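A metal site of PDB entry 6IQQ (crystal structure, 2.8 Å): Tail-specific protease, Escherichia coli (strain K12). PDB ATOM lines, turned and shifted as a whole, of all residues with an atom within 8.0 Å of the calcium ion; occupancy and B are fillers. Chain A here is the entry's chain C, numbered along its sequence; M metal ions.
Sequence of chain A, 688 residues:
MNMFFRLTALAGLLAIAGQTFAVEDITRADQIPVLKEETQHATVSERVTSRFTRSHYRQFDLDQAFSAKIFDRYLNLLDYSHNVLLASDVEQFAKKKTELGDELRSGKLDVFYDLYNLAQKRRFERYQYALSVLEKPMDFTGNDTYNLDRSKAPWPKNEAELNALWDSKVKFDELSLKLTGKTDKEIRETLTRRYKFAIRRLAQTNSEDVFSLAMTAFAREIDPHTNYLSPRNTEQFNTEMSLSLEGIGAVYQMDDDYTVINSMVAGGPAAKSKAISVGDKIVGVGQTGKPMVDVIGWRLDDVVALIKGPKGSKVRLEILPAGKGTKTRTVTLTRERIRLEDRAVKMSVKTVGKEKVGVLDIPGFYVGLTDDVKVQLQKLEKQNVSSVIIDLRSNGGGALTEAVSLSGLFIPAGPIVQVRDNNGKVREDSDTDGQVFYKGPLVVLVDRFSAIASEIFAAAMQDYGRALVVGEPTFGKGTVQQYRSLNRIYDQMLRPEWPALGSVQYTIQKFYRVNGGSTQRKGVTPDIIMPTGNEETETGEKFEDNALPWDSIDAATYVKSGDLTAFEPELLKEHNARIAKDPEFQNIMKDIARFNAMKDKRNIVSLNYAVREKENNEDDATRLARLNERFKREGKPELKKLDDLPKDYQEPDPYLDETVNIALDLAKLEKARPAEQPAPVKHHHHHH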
ATOM      1  N   VAL A 404      23.399 -19.482   9.470  1.00  0.00           N
ATOM      2  CA  VAL A 404      22.505 -20.566   8.962  1.00  0.00           C
ATOM      3  C   VAL A 404      21.191 -20.544   9.744  1.00  0.00           C
ATOM      4  O   VAL A 404      20.114 -20.606   9.138  1.00  0.00           O
ATOM      5  CB  VAL A 404      23.240 -21.901   9.091  1.00  0.00           C
ATOM      6  CG1 VAL A 404      22.312 -23.054   8.820  1.00  0.00           C
ATOM      7  CG2 VAL A 404      24.434 -21.926   8.161  1.00  0.00           C
ATOM      8  N   SER A 405      21.242 -20.415  11.056  1.00  0.00           N
ATOM      9  CA  SER A 405      19.988 -20.412  11.826  1.00  0.00           C
ATOM     10  C   SER A 405      19.209 -19.180  11.439  1.00  0.00           C
ATOM     11  O   SER A 405      17.974 -19.296  11.236  1.00  0.00           O
ATOM     12  CB  SER A 405      20.248 -20.469  13.304  1.00  0.00           C
ATOM     13  OG  SER A 405      21.130 -19.454  13.722  1.00  0.00           O
ATOM     14  N   LEU A 406      19.896 -18.021  11.367  1.00  0.00           N
ATOM     15  CA  LEU A 406      19.240 -16.723  11.099  1.00  0.00           C
ATOM     16  C   LEU A 406      18.608 -16.806   9.716  1.00  0.00           C
ATOM     17  O   LEU A 406      17.459 -16.394   9.597  1.00  0.00           O
ATOM     18  CB  LEU A 406      20.230 -15.563  11.192  1.00  0.00           C
ATOM     19  CG  LEU A 406      19.634 -14.198  10.902  1.00  0.00           C
ATOM     20  CD1 LEU A 406      18.731 -13.751  12.029  1.00  0.00           C
ATOM     21  CD2 LEU A 406      20.707 -13.165  10.650  1.00  0.00           C
ATOM     22  N   SER A 407      19.342 -17.310   8.715  1.00  0.00           N
ATOM     23  CA  SER A 407      18.817 -17.560   7.347  1.00  0.00           C
ATOM     24  C   SER A 407      17.516 -18.334   7.491  1.00  0.00           C
ATOM     25  O   SER A 407      16.543 -17.952   6.835  1.00  0.00           O
ATOM     26  CB  SER A 407      19.746 -18.329   6.449  1.00  0.00           C
ATOM     27  OG  SER A 407      20.868 -17.555   6.071  1.00  0.00           O
ATOM     28  N   GLY A 408      17.542 -19.378   8.313  1.00  0.00           N
ATOM     29  CA  GLY A 408      16.443 -20.354   8.448  1.00  0.00           C
ATOM     30  C   GLY A 408      15.185 -19.774   9.049  1.00  0.00           C
ATOM     31  O   GLY A 408      14.178 -20.480   9.018  1.00  0.00           O
ATOM     32  N   LEU A 409      15.247 -18.574   9.651  1.00  0.00           N
ATOM     33  CA  LEU A 409      14.060 -17.971  10.304  1.00  0.00           C
ATOM     34  C   LEU A 409      13.083 -17.525   9.238  1.00  0.00           C
ATOM     35  O   LEU A 409      11.941 -17.265   9.608  1.00  0.00           O
ATOM     36  CB  LEU A 409      14.425 -16.784  11.211  1.00  0.00           C
ATOM     37  CG  LEU A 409      15.126 -17.130  12.514  1.00  0.00           C
ATOM     38  CD1 LEU A 409      15.277 -15.881  13.356  1.00  0.00           C
ATOM     39  CD2 LEU A 409      14.381 -18.173  13.318  1.00  0.00           C
ATOM     40  N   PHE A 410      13.519 -17.415   7.979  1.00  0.00           N
ATOM     41  CA  PHE A 410      12.721 -16.717   6.936  1.00  0.00           C
ATOM     42  C   PHE A 410      12.354 -17.715   5.846  1.00  0.00           C
ATOM     43  O   PHE A 410      11.565 -17.349   4.997  1.00  0.00           O
ATOM     44  CB  PHE A 410      13.456 -15.478   6.403  1.00  0.00           C
ATOM     45  CG  PHE A 410      13.910 -14.515   7.484  1.00  0.00           C
ATOM     46  CD1 PHE A 410      13.029 -13.634   8.071  1.00  0.00           C
ATOM     47  CD2 PHE A 410      15.219 -14.520   7.933  1.00  0.00           C
ATOM     48  CE1 PHE A 410      13.450 -12.791   9.085  1.00  0.00           C
ATOM     49  CE2 PHE A 410      15.644 -13.669   8.943  1.00  0.00           C
ATOM     50  CZ  PHE A 410      14.745 -12.808   9.521  1.00  0.00           C
ATOM     51  N   ILE A 411      12.966 -18.899   5.845  1.00  0.00           N
ATOM     52  CA  ILE A 411      12.614 -20.038   4.943  1.00  0.00           C
ATOM     53  C   ILE A 411      12.039 -21.188   5.776  1.00  0.00           C
ATOM     54  O   ILE A 411      12.407 -21.369   6.942  1.00  0.00           O
ATOM     55  CB  ILE A 411      13.795 -20.471   4.046  1.00  0.00           C
ATOM     56  CG1 ILE A 411      14.970 -21.079   4.813  1.00  0.00           C
ATOM     57  CG2 ILE A 411      14.279 -19.328   3.189  1.00  0.00           C
ATOM     58  CD1 ILE A 411      15.866 -21.931   3.940  1.00  0.00           C
ATOM     59  N   PRO A 412      11.114 -22.035   5.233  1.00  0.00           N
ATOM     60  CA  PRO A 412      10.713 -23.251   5.934  1.00  0.00           C
ATOM     61  C   PRO A 412      11.958 -24.111   6.282  1.00  0.00           C
ATOM     62  O   PRO A 412      12.235 -24.243   7.455  1.00  0.00           O
ATOM     63  CB  PRO A 412       9.753 -23.935   4.958  1.00  0.00           C
ATOM     64  CG  PRO A 412       9.228 -22.791   4.115  1.00  0.00           C
ATOM     65  CD  PRO A 412      10.431 -21.897   3.929  1.00  0.00           C
ATOM     66  N   ALA A 413      12.674 -24.634   5.271  1.00  0.00           N
ATOM     67  CA  ALA A 413      13.853 -25.485   5.489  1.00  0.00           C
ATOM     68  C   ALA A 413      14.570 -25.728   4.180  1.00  0.00           C
ATOM     69  O   ALA A 413      13.889 -25.793   3.153  1.00  0.00           O
ATOM     70  CB  ALA A 413      13.429 -26.822   6.017  1.00  0.00           C
ATOM     71  N   GLY A 414      15.867 -25.955   4.261  1.00  0.00           N
ATOM     72  CA  GLY A 414      16.692 -26.064   3.060  1.00  0.00           C
ATOM     73  C   GLY A 414      18.157 -25.916   3.398  1.00  0.00           C
ATOM     74  O   GLY A 414      18.491 -25.659   4.557  1.00  0.00           O
ATOM     75  N   ILE A 416      21.683 -23.744   3.271  1.00  0.00           N
ATOM     76  CA  ILE A 416      21.970 -22.295   3.377  1.00  0.00           C
ATOM     77  C   ILE A 416      23.300 -22.023   2.716  1.00  0.00           C
ATOM     78  O   ILE A 416      23.381 -21.031   2.016  1.00  0.00           O
ATOM     79  CB  ILE A 416      21.930 -21.822   4.846  1.00  0.00           C
ATOM     80  CG1 ILE A 416      20.594 -22.152   5.513  1.00  0.00           C
ATOM     81  CG2 ILE A 416      22.236 -20.347   4.948  1.00  0.00           C
ATOM     82  CD1 ILE A 416      19.364 -21.599   4.796  1.00  0.00           C
ATOM     83  N   ASP A 431      19.079 -25.508   7.572  1.00  0.00           N
ATOM     84  CA  ASP A 431      17.942 -25.219   8.475  1.00  0.00           C
ATOM     85  C   ASP A 431      16.915 -26.304   8.165  1.00  0.00           C
ATOM     86  O   ASP A 431      16.576 -26.509   6.927  1.00  0.00           O
ATOM     87  CB  ASP A 431      17.384 -23.822   8.238  1.00  0.00           C
ATOM     88  CG  ASP A 431      16.167 -23.485   9.087  1.00  0.00           C
ATOM     89  OD1 ASP A 431      16.327 -23.091  10.314  1.00  0.00           O
ATOM     90  OD2 ASP A 431      15.063 -23.571   8.499  1.00  0.00           O
ATOM     91  N   THR A 432      16.486 -27.015   9.224  1.00  0.00           N
ATOM     92  CA  THR A 432      15.766 -28.314   9.099  1.00  0.00           C
ATOM     93  C   THR A 432      14.387 -28.273   9.770  1.00  0.00           C
ATOM     94  O   THR A 432      13.557 -29.083   9.332  1.00  0.00           O
ATOM     95  CB  THR A 432      16.614 -29.452   9.667  1.00  0.00           C
ATOM     96  OG1 THR A 432      16.787 -29.106  11.036  1.00  0.00           O
ATOM     97  CG2 THR A 432      17.946 -29.625   8.961  1.00  0.00           C
ATOM     98  N   ASP A 433      14.144 -27.387  10.752  1.00  0.00           N
ATOM     99  CA  ASP A 433      12.761 -27.082  11.210  1.00  0.00           C
ATOM    100  C   ASP A 433      12.054 -26.510   9.998  1.00  0.00           C
ATOM    101  O   ASP A 433      12.654 -25.653   9.354  1.00  0.00           O
ATOM    102  CB  ASP A 433      12.677 -26.140  12.431  1.00  0.00           C
ATOM    103  CG  ASP A 433      12.773 -24.623  12.246  1.00  0.00           C
ATOM    104  OD1 ASP A 433      12.877 -24.127  11.086  1.00  0.00           O
ATOM    105  OD2 ASP A 433      12.740 -23.924  13.303  1.00  0.00           O
ATOM    106  N   GLY A 434      10.866 -26.998   9.654  1.00  0.00           N
ATOM    107  CA  GLY A 434      10.125 -26.514   8.481  1.00  0.00           C
ATOM    108  C   GLY A 434       9.293 -25.296   8.834  1.00  0.00           C
ATOM    109  O   GLY A 434       8.229 -25.174   8.219  1.00  0.00           O
ATOM    110  N   GLN A 435       9.813 -24.432   9.718  1.00  0.00           N
ATOM    111  CA  GLN A 435       9.149 -23.262  10.368  1.00  0.00           C
ATOM    112  C   GLN A 435       9.573 -21.916   9.714  1.00  0.00           C
ATOM    113  O   GLN A 435      10.776 -21.739   9.350  1.00  0.00           O
ATOM    114  CB  GLN A 435       9.454 -23.224  11.880  1.00  0.00           C
ATOM    115  CG  GLN A 435       9.135 -24.513  12.619  1.00  0.00           C
ATOM    116  CD  GLN A 435       7.714 -24.985  12.434  1.00  0.00           C
ATOM    117  OE1 GLN A 435       6.767 -24.398  12.959  1.00  0.00           O
ATOM    118  NE2 GLN A 435       7.537 -26.090  11.703  1.00  0.00           N
ATOM    119  N   VAL A 436       8.646 -20.961   9.647  1.00  0.00           N
ATOM    120  CA  VAL A 436       8.937 -19.566   9.234  1.00  0.00           C
ATOM    121  C   VAL A 436       8.463 -18.615  10.327  1.00  0.00           C
ATOM    122  O   VAL A 436       7.292 -18.615  10.574  1.00  0.00           O
ATOM    123  CB  VAL A 436       8.260 -19.238   7.878  1.00  0.00           C
ATOM    124  CG1 VAL A 436       8.741 -17.901   7.369  1.00  0.00           C
ATOM    125  CG2 VAL A 436       8.549 -20.313   6.845  1.00  0.00           C
ATOM    126  N   PHE A 437       9.373 -17.866  10.959  1.00  0.00           N
ATOM    127  CA  PHE A 437       9.096 -16.987  12.128  1.00  0.00           C
ATOM    128  C   PHE A 437       8.771 -15.549  11.716  1.00  0.00           C
ATOM    129  O   PHE A 437       8.563 -14.707  12.613  1.00  0.00           O
ATOM    130  CB  PHE A 437      10.268 -17.026  13.112  1.00  0.00           C
ATOM    131  CG  PHE A 437      10.330 -18.336  13.828  1.00  0.00           C
ATOM    132  CD1 PHE A 437      10.766 -19.480  13.174  1.00  0.00           C
ATOM    133  CD2 PHE A 437       9.918 -18.433  15.140  1.00  0.00           C
ATOM    134  CE1 PHE A 437      10.842 -20.692  13.846  1.00  0.00           C
ATOM    135  CE2 PHE A 437       9.993 -19.645  15.812  1.00  0.00           C
ATOM    136  CZ  PHE A 437      10.444 -20.771  15.158  1.00  0.00           C
HETATM  137 CA    CA M   1      13.003 -22.534   9.228  1.00  0.00          CA
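Six residues have an atom within 4 Å of the calcium ion: Gly 408, Ile 411, Pro 412, Asp 431, Asp 433 and Gln 435. The nearest printed residue that does not touch the calcium ion is Ala 413 (4.5 Å).
N of Gly 414 lies within hydrogen-bond range of O of Asp 431.
O of Gln 435 binds the calcium ion (2.4 Å). The backbone carbonyl oxygen (O) of Gly 408 is bound to the calcium ion (2.4 Å). The calcium ion is bound by OD2 of Asp 431, at 2.4 Å. The side-chain carboxylate (OD1) of Asp 433 is bound to the calcium ion, 2.5 Å away. O of Pro 412 binds the calcium ion (2.6 Å). The backbone carbonyl oxygen (O) of Ile 411 binds the calcium ion. The calcium ion has six donor atoms within binding distance. Slightly farther from the calcium ion lies the backbone carbonyl oxygen (O) of Asp 433 (3.1 Å).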
